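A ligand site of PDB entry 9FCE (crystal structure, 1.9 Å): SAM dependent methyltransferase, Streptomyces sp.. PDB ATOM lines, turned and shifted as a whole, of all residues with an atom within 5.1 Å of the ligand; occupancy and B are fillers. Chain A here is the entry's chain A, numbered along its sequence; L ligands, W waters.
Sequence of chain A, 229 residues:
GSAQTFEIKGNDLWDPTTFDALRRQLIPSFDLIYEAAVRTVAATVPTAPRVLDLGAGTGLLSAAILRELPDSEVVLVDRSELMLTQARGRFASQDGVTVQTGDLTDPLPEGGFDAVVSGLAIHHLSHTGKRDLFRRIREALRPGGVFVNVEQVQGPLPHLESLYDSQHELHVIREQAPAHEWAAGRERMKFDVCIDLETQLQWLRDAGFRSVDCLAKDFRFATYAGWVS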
ATOM      1  N   PHE A  19     -13.111 -34.427 -13.647  1.00  0.00           N
ATOM      2  CA  PHE A  19     -13.619 -33.322 -14.448  1.00  0.00           C
ATOM      3  C   PHE A  19     -12.720 -32.106 -14.260  1.00  0.00           C
ATOM      4  O   PHE A  19     -12.255 -31.525 -15.229  1.00  0.00           O
ATOM      5  CB  PHE A  19     -15.077 -33.051 -14.060  1.00  0.00           C
ATOM      6  CG  PHE A  19     -15.732 -31.876 -14.760  1.00  0.00           C
ATOM      7  CD1 PHE A  19     -16.237 -31.994 -16.056  1.00  0.00           C
ATOM      8  CD2 PHE A  19     -15.840 -30.641 -14.125  1.00  0.00           C
ATOM      9  CE1 PHE A  19     -16.829 -30.915 -16.686  1.00  0.00           C
ATOM     10  CE2 PHE A  19     -16.432 -29.565 -14.768  1.00  0.00           C
ATOM     11  CZ  PHE A  19     -16.934 -29.709 -16.043  1.00  0.00           C
ATOM     12  N   ARG A  23     -10.733 -29.957 -16.833  1.00  0.00           N
ATOM     13  CA  ARG A  23     -10.936 -28.523 -17.018  1.00  0.00           C
ATOM     14  C   ARG A  23      -9.598 -27.784 -17.045  1.00  0.00           C
ATOM     15  O   ARG A  23      -9.431 -26.866 -17.851  1.00  0.00           O
ATOM     16  CB  ARG A  23     -11.868 -27.896 -15.954  1.00  0.00           C
ATOM     17  CG  ARG A  23     -13.304 -28.408 -15.989  1.00  0.00           C
ATOM     18  CD  ARG A  23     -13.973 -28.278 -17.359  1.00  0.00           C
ATOM     19  NE  ARG A  23     -14.280 -26.880 -17.677  1.00  0.00           N
ATOM     20  CZ  ARG A  23     -14.637 -26.414 -18.867  1.00  0.00           C
ATOM     21  NH1 ARG A  23     -14.561 -27.178 -19.938  1.00  0.00           N
ATOM     22  NH2 ARG A  23     -15.018 -25.149 -18.975  1.00  0.00           N
ATOM     23  N   TYR A  34      -9.719 -18.629 -11.781  1.00  0.00           N
ATOM     24  CA  TYR A  34     -10.746 -19.012 -10.821  1.00  0.00           C
ATOM     25  C   TYR A  34     -10.373 -18.460  -9.446  1.00  0.00           C
ATOM     26  O   TYR A  34     -11.235 -17.904  -8.761  1.00  0.00           O
ATOM     27  CB  TYR A  34     -11.014 -20.523 -10.828  1.00  0.00           C
ATOM     28  CG  TYR A  34     -11.968 -20.914 -11.951  1.00  0.00           C
ATOM     29  CD1 TYR A  34     -13.342 -20.956 -11.762  1.00  0.00           C
ATOM     30  CD2 TYR A  34     -11.501 -21.183 -13.228  1.00  0.00           C
ATOM     31  CE1 TYR A  34     -14.217 -21.292 -12.793  1.00  0.00           C
ATOM     32  CE2 TYR A  34     -12.352 -21.528 -14.272  1.00  0.00           C
ATOM     33  CZ  TYR A  34     -13.710 -21.570 -14.054  1.00  0.00           C
ATOM     34  OH  TYR A  34     -14.532 -21.907 -15.094  1.00  0.00           O
ATOM     35  N   ASP A  53     -24.376 -17.801  -8.281  1.00  0.00           N
ATOM     36  CA  ASP A  53     -23.502 -18.357  -9.312  1.00  0.00           C
ATOM     37  C   ASP A  53     -24.325 -18.593 -10.572  1.00  0.00           C
ATOM     38  O   ASP A  53     -25.134 -19.511 -10.621  1.00  0.00           O
ATOM     39  CB  ASP A  53     -22.806 -19.624  -8.816  1.00  0.00           C
ATOM     40  CG  ASP A  53     -21.745 -20.213  -9.733  1.00  0.00           C
ATOM     41  OD1 ASP A  53     -21.544 -19.659 -10.841  1.00  0.00           O
ATOM     42  OD2 ASP A  53     -21.132 -21.228  -9.351  1.00  0.00           O
ATOM     43  N   LEU A  54     -24.093 -17.755 -11.608  1.00  0.00           N
ATOM     44  CA  LEU A  54     -24.893 -17.776 -12.828  1.00  0.00           C
ATOM     45  C   LEU A  54     -24.212 -18.635 -13.891  1.00  0.00           C
ATOM     46  O   LEU A  54     -23.028 -18.466 -14.169  1.00  0.00           O
ATOM     47  CB  LEU A  54     -25.090 -16.349 -13.349  1.00  0.00           C
ATOM     48  CG  LEU A  54     -26.016 -15.446 -12.527  1.00  0.00           C
ATOM     49  CD1 LEU A  54     -26.155 -14.108 -13.208  1.00  0.00           C
ATOM     50  CD2 LEU A  54     -27.377 -16.064 -12.313  1.00  0.00           C
ATOM     51  N   GLY A  55     -25.000 -19.508 -14.527  1.00  0.00           N
ATOM     52  CA  GLY A  55     -24.471 -20.555 -15.392  1.00  0.00           C
ATOM     53  C   GLY A  55     -23.513 -21.462 -14.625  1.00  0.00           C
ATOM     54  O   GLY A  55     -22.402 -21.703 -15.092  1.00  0.00           O
ATOM     55  N   ALA A  56     -23.963 -21.960 -13.466  1.00  0.00           N
ATOM     56  CA  ALA A  56     -23.092 -22.587 -12.467  1.00  0.00           C
ATOM     57  C   ALA A  56     -22.471 -23.885 -12.961  1.00  0.00           C
ATOM     58  O   ALA A  56     -21.414 -24.288 -12.474  1.00  0.00           O
ATOM     59  CB  ALA A  56     -23.881 -22.823 -11.204  1.00  0.00           C
ATOM     60  N   GLY A  57     -23.147 -24.569 -13.898  1.00  0.00           N
ATOM     61  CA  GLY A  57     -22.689 -25.868 -14.378  1.00  0.00           C
ATOM     62  C   GLY A  57     -22.638 -26.892 -13.247  1.00  0.00           C
ATOM     63  O   GLY A  57     -23.629 -27.073 -12.552  1.00  0.00           O
ATOM     64  N   THR A  58     -21.475 -27.517 -13.053  1.00  0.00           N
ATOM     65  CA  THR A  58     -21.274 -28.506 -11.995  1.00  0.00           C
ATOM     66  C   THR A  58     -21.060 -27.804 -10.651  1.00  0.00           C
ATOM     67  O   THR A  58     -21.051 -28.462  -9.615  1.00  0.00           O
ATOM     68  CB  THR A  58     -20.109 -29.448 -12.314  1.00  0.00           C
ATOM     69  OG1 THR A  58     -18.878 -28.737 -12.256  1.00  0.00           O
ATOM     70  CG2 THR A  58     -20.211 -30.086 -13.680  1.00  0.00           C
ATOM     71  N   LEU A  60     -18.329 -25.515 -10.071  1.00  0.00           N
ATOM     72  CA  LEU A  60     -16.893 -25.447  -9.857  1.00  0.00           C
ATOM     73  C   LEU A  60     -16.495 -24.106  -9.217  1.00  0.00           C
ATOM     74  O   LEU A  60     -15.590 -24.061  -8.390  1.00  0.00           O
ATOM     75  CB  LEU A  60     -16.267 -25.660 -11.236  1.00  0.00           C
ATOM     76  CG  LEU A  60     -14.735 -25.696 -11.334  1.00  0.00           C
ATOM     77  CD1 LEU A  60     -14.058 -26.338 -10.141  1.00  0.00           C
ATOM     78  CD2 LEU A  60     -14.369 -26.420 -12.625  1.00  0.00           C
ATOM     79  N   LEU A  61     -17.191 -23.020  -9.580  1.00  0.00           N
ATOM     80  CA  LEU A  61     -16.890 -21.700  -9.057  1.00  0.00           C
ATOM     81  C   LEU A  61     -17.494 -21.529  -7.659  1.00  0.00           C
ATOM     82  O   LEU A  61     -16.870 -20.950  -6.778  1.00  0.00           O
ATOM     83  CB  LEU A  61     -17.386 -20.639 -10.038  1.00  0.00           C
ATOM     84  CG  LEU A  61     -17.026 -19.182  -9.739  1.00  0.00           C
ATOM     85  CD1 LEU A  61     -15.552 -18.956  -9.483  1.00  0.00           C
ATOM     86  CD2 LEU A  61     -17.502 -18.299 -10.876  1.00  0.00           C
ATOM     87  N   ASP A  78     -28.580 -22.583 -13.507  1.00  0.00           N
ATOM     88  CA  ASP A  78     -28.163 -23.121 -14.794  1.00  0.00           C
ATOM     89  C   ASP A  78     -29.386 -23.668 -15.540  1.00  0.00           C
ATOM     90  O   ASP A  78     -30.327 -24.142 -14.917  1.00  0.00           O
ATOM     91  CB  ASP A  78     -27.100 -24.177 -14.612  1.00  0.00           C
ATOM     92  CG  ASP A  78     -26.227 -24.421 -15.829  1.00  0.00           C
ATOM     93  OD1 ASP A  78     -26.757 -24.910 -16.842  1.00  0.00           O
ATOM     94  OD2 ASP A  78     -25.022 -24.098 -15.754  1.00  0.00           O
ATOM     95  N   ARG A  79     -29.362 -23.598 -16.871  1.00  0.00           N
ATOM     96  CA  ARG A  79     -30.504 -24.047 -17.669  1.00  0.00           C
ATOM     97  C   ARG A  79     -30.440 -25.557 -17.870  1.00  0.00           C
ATOM     98  O   ARG A  79     -31.449 -26.156 -18.240  1.00  0.00           O
ATOM     99  CB  ARG A  79     -30.576 -23.339 -19.033  1.00  0.00           C
ATOM    100  CG  ARG A  79     -29.471 -23.699 -20.018  1.00  0.00           C
ATOM    101  CD  ARG A  79     -29.569 -22.902 -21.304  1.00  0.00           C
ATOM    102  NE  ARG A  79     -28.453 -23.231 -22.195  1.00  0.00           N
ATOM    103  CZ  ARG A  79     -28.202 -22.665 -23.374  1.00  0.00           C
ATOM    104  NH1 ARG A  79     -28.966 -21.687 -23.836  1.00  0.00           N
ATOM    105  NH2 ARG A  79     -27.157 -23.068 -24.086  1.00  0.00           N
ATOM    106  N   SER A  80     -29.263 -26.150 -17.642  1.00  0.00           N
ATOM    107  CA  SER A  80     -29.032 -27.572 -17.874  1.00  0.00           C
ATOM    108  C   SER A  80     -29.245 -28.365 -16.586  1.00  0.00           C
ATOM    109  O   SER A  80     -28.480 -28.234 -15.640  1.00  0.00           O
ATOM    110  CB  SER A  80     -27.639 -27.804 -18.419  1.00  0.00           C
ATOM    111  OG  SER A  80     -27.382 -29.190 -18.595  1.00  0.00           O
ATOM    112  N   MET A  83     -26.358 -30.794 -15.760  1.00  0.00           N
ATOM    113  CA  MET A  83     -25.255 -30.143 -15.070  1.00  0.00           C
ATOM    114  C   MET A  83     -25.582 -29.968 -13.586  1.00  0.00           C
ATOM    115  O   MET A  83     -24.758 -30.286 -12.733  1.00  0.00           O
ATOM    116  CB  MET A  83     -24.957 -28.768 -15.673  1.00  0.00           C
ATOM    117  CG  MET A  83     -24.317 -28.834 -17.044  1.00  0.00           C
ATOM    118  SD  MET A  83     -22.614 -29.405 -16.979  1.00  0.00           S
ATOM    119  CE  MET A  83     -21.663 -27.887 -17.166  1.00  0.00           C
ATOM    120  N   GLY A 102     -32.750 -22.436 -14.380  1.00  0.00           N
ATOM    121  CA  GLY A 102     -33.073 -21.102 -14.841  1.00  0.00           C
ATOM    122  C   GLY A 102     -32.173 -20.681 -16.007  1.00  0.00           C
ATOM    123  O   GLY A 102     -31.072 -21.211 -16.155  1.00  0.00           O
ATOM    124  N   ASP A 103     -32.666 -19.740 -16.813  1.00  0.00           N
ATOM    125  CA  ASP A 103     -31.894 -19.179 -17.919  1.00  0.00           C
ATOM    126  C   ASP A 103     -31.306 -17.842 -17.483  1.00  0.00           C
ATOM    127  O   ASP A 103     -31.922 -17.132 -16.696  1.00  0.00           O
ATOM    128  CB  ASP A 103     -32.753 -19.023 -19.159  1.00  0.00           C
ATOM    129  CG  ASP A 103     -31.990 -18.917 -20.465  1.00  0.00           C
ATOM    130  OD1 ASP A 103     -31.401 -17.832 -20.722  1.00  0.00           O
ATOM    131  OD2 ASP A 103     -31.951 -19.929 -21.198  1.00  0.00           O
ATOM    132  N   LEU A 104     -30.136 -17.483 -18.014  1.00  0.00           N
ATOM    133  CA  LEU A 104     -29.503 -16.211 -17.686  1.00  0.00           C
ATOM    134  C   LEU A 104     -30.412 -15.040 -18.045  1.00  0.00           C
ATOM    135  O   LEU A 104     -30.339 -13.992 -17.406  1.00  0.00           O
ATOM    136  CB  LEU A 104     -28.142 -16.093 -18.374  1.00  0.00           C
ATOM    137  CG  LEU A 104     -27.053 -17.068 -17.938  1.00  0.00           C
ATOM    138  CD1 LEU A 104     -25.863 -17.030 -18.885  1.00  0.00           C
ATOM    139  CD2 LEU A 104     -26.579 -16.812 -16.525  1.00  0.00           C
ATOM    140  N   THR A 105     -31.258 -15.218 -19.078  1.00  0.00           N
ATOM    141  CA  THR A 105     -32.150 -14.173 -19.541  1.00  0.00           C
ATOM    142  C   THR A 105     -33.416 -14.090 -18.671  1.00  0.00           C
ATOM    143  O   THR A 105     -34.190 -13.157 -18.833  1.00  0.00           O
ATOM    144  CB  THR A 105     -32.517 -14.418 -21.012  1.00  0.00           C
ATOM    145  OG1 THR A 105     -33.116 -15.701 -21.088  1.00  0.00           O
ATOM    146  CG2 THR A 105     -31.305 -14.368 -21.926  1.00  0.00           C
ATOM    147  N   GLY A 119     -18.842 -18.129 -14.510  1.00  0.00           N
ATOM    148  CA  GLY A 119     -17.684 -18.678 -15.185  1.00  0.00           C
ATOM    149  C   GLY A 119     -18.080 -19.288 -16.520  1.00  0.00           C
ATOM    150  O   GLY A 119     -18.853 -20.231 -16.549  1.00  0.00           O
ATOM    151  N   LEU A 120     -17.555 -18.711 -17.609  1.00  0.00           N
ATOM    152  CA  LEU A 120     -17.601 -19.289 -18.942  1.00  0.00           C
ATOM    153  C   LEU A 120     -19.044 -19.571 -19.367  1.00  0.00           C
ATOM    154  O   LEU A 120     -19.315 -20.605 -19.959  1.00  0.00           O
ATOM    155  CB  LEU A 120     -16.739 -20.552 -18.990  1.00  0.00           C
ATOM    156  CG  LEU A 120     -15.291 -20.377 -18.549  1.00  0.00           C
ATOM    157  CD1 LEU A 120     -14.556 -21.707 -18.618  1.00  0.00           C
ATOM    158  CD2 LEU A 120     -14.563 -19.304 -19.359  1.00  0.00           C
ATOM    159  N   ALA A 121     -19.936 -18.600 -19.124  1.00  0.00           N
ATOM    160  CA  ALA A 121     -21.363 -18.754 -19.373  1.00  0.00           C
ATOM    161  C   ALA A 121     -21.925 -17.579 -20.178  1.00  0.00           C
ATOM    162  O   ALA A 121     -22.726 -17.771 -21.106  1.00  0.00           O
ATOM    163  CB  ALA A 121     -22.077 -18.890 -18.052  1.00  0.00           C
ATOM    164  N   HIS A 124     -22.292 -16.826 -24.064  1.00  0.00           N
ATOM    165  CA  HIS A 124     -23.293 -17.502 -24.875  1.00  0.00           C
ATOM    166  C   HIS A 124     -24.527 -16.638 -25.135  1.00  0.00           C
ATOM    167  O   HIS A 124     -25.367 -17.026 -25.946  1.00  0.00           O
ATOM    168  CB  HIS A 124     -23.770 -18.809 -24.241  1.00  0.00           C
ATOM    169  CG  HIS A 124     -22.661 -19.779 -24.153  1.00  0.00           C
ATOM    170  ND1 HIS A 124     -22.114 -20.142 -22.947  1.00  0.00           N
ATOM    171  CD2 HIS A 124     -21.985 -20.431 -25.098  1.00  0.00           C
ATOM    172  CE1 HIS A 124     -21.157 -21.025 -23.158  1.00  0.00           C
ATOM    173  NE2 HIS A 124     -21.044 -21.194 -24.453  1.00  0.00           N
ATOM    174  N   LEU A 125     -24.644 -15.493 -24.460  1.00  0.00           N
ATOM    175  CA  LEU A 125     -25.770 -14.578 -24.664  1.00  0.00           C
ATOM    176  C   LEU A 125     -25.465 -13.653 -25.838  1.00  0.00           C
ATOM    177  O   LEU A 125     -24.299 -13.358 -26.092  1.00  0.00           O
ATOM    178  CB  LEU A 125     -26.036 -13.723 -23.429  1.00  0.00           C
ATOM    179  CG  LEU A 125     -26.444 -14.476 -22.154  1.00  0.00           C
ATOM    180  CD1 LEU A 125     -26.578 -13.439 -21.042  1.00  0.00           C
ATOM    181  CD2 LEU A 125     -27.726 -15.274 -22.355  1.00  0.00           C
HETATM  182  N1  LIG L   1     -19.718 -22.026 -14.621  1.00  0.00           N
HETATM  183  C1  LIG L   1     -19.207 -23.421 -14.745  1.00  0.00           C
HETATM  184  C2  LIG L   1     -17.680 -23.418 -14.632  1.00  0.00           C
HETATM  185  O1  LIG L   1     -17.112 -24.534 -14.602  1.00  0.00           O
HETATM  186  O2  LIG L   1     -17.120 -22.297 -14.553  1.00  0.00           O
HETATM  187  C3  LIG L   1     -19.642 -24.062 -16.070  1.00  0.00           C
HETATM  188  C4  LIG L   1     -19.282 -23.301 -17.346  1.00  0.00           C
HETATM  189  S1  LIG L   1     -19.895 -24.174 -18.827  1.00  0.00           S
HETATM  190  C5  LIG L   1     -18.639 -23.836 -20.061  1.00  0.00           C
HETATM  191  C6  LIG L   1     -21.257 -23.065 -19.293  1.00  0.00           C
HETATM  192  C7  LIG L   1     -22.508 -23.284 -18.462  1.00  0.00           C
HETATM  193  O3  LIG L   1     -23.417 -22.196 -18.708  1.00  0.00           O
HETATM  194  C8  LIG L   1     -23.299 -24.578 -18.741  1.00  0.00           C
HETATM  195  O4  LIG L   1     -23.605 -25.258 -17.528  1.00  0.00           O
HETATM  196  C9  LIG L   1     -24.560 -24.092 -19.452  1.00  0.00           C
HETATM  197  O5  LIG L   1     -25.695 -24.869 -19.155  1.00  0.00           O
HETATM  198  C10 LIG L   1     -24.724 -22.696 -18.869  1.00  0.00           C
HETATM  199  N2  LIG L   1     -25.477 -21.775 -19.705  1.00  0.00           N
HETATM  200  C11 LIG L   1     -25.155 -21.323 -20.957  1.00  0.00           C
HETATM  201  N3  LIG L   1     -26.027 -20.486 -21.449  1.00  0.00           N
HETATM  202  C12 LIG L   1     -27.000 -20.377 -20.463  1.00  0.00           C
HETATM  203  C13 LIG L   1     -28.192 -19.632 -20.374  1.00  0.00           C
HETATM  204  N4  LIG L   1     -28.637 -18.829 -21.326  1.00  0.00           N
HETATM  205  N5  LIG L   1     -28.920 -19.749 -19.227  1.00  0.00           N
HETATM  206  C14 LIG L   1     -28.459 -20.557 -18.259  1.00  0.00           C
HETATM  207  N6  LIG L   1     -27.360 -21.298 -18.229  1.00  0.00           N
HETATM  208  C15 LIG L   1     -26.659 -21.168 -19.371  1.00  0.00           C
HETATM  209  O   HOH W   1     -18.175 -22.368 -22.780  1.00  0.00           O
HETATM  210  O   HOH W   2     -20.754 -19.952 -13.218  1.00  0.00           O
HETATM  211  O   HOH W   3     -14.788 -24.596 -16.190  1.00  0.00           O
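O of Gly 55 is in hydrogen-bond range of N1 of the ligand, 2.7 Å away.
The backbone NH (N) of Arg 79 is in hydrogen-bond range of a nitrogen (N6) of the ligand.
The backbone carbonyl oxygen (O) of Gly 119 lies within hydrogen-bond range of a nitrogen (N1) of the ligand (2.8 Å).
The backbone NH (N) of Leu 104 lies within hydrogen-bond range of a nitrogen (N5) of the ligand (2.8 Å).
OD1 of Asp 78 lies within hydrogen-bond range of O5 of the ligand (2.5 Å).
The side-chain hydroxyl (OH) of Tyr 34 sits at hydrogen-bond distance from an oxygen (O2) of the ligand.
OD1 of Asp 103 is in hydrogen-bond range of N4 of the ligand (3.0 Å).
The backbone carbonyl oxygen (O) of Ala 121 sits at hydrogen-bond distance from a ring nitrogen (ND1) of His 124 (3.1 Å).
The side-chain carboxylate (OD1) of Asp 78 sits at hydrogen-bond distance from the backbone NH (N) of Ser 80.
The backbone NH (N) of Met 83 sits at hydrogen-bond distance from the side-chain hydroxyl (OG) of Ser 80 (3.4 Å).
The backbone NH (N) of Arg 79 lies within hydrogen-bond range of the backbone carbonyl oxygen (O) of Gly 102 (3.0 Å).
The backbone NH of Gly 57 is in hydrogen-bond range of the side-chain carboxylate of Asp 78 (2.7 Å).
OD1 of Asp 103 lies within hydrogen-bond range of OG1 of Thr 105, 2.8 Å away.
N of Ala 56 is in hydrogen-bond range of OD2 of Asp 78 (3.3 Å).
The backbone carbonyl oxygen of Asp 78 lies within hydrogen-bond range of the backbone NH of Gly 102 (3.0 Å).
O of Leu 120 lies close to S1 of the ligand (3.8 Å).
Merely in contact with the ligand: Ala 56 (3.3 Å), Met 83 (3.3 Å), Gly 57 (3.3 Å), Gly 102 (3.4 Å), Ser 80 (3.6 Å), Ala 121 (3.6 Å), Leu 60 (3.6 Å), Leu 125 (3.8 Å) and His 124 (3.8 Å).
Hydrophobic or aromatic side chains within 4 Å of the ligand: Tyr 34, Leu 60, Met 83, Leu 104, Leu 120, Ala 121, His 124 and Leu 125.
Along chain A the residues within 4 Å of the ligand span positions 34 to 125.
The nearest printed residue that does not touch the ligand is Arg 23 (4.002 Å).
Water W3 lies within hydrogen-bond range of NE of Arg 23 (2.8 Å), O1 of the ligand (2.8 Å) and OH of Tyr 34 (2.9 Å).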
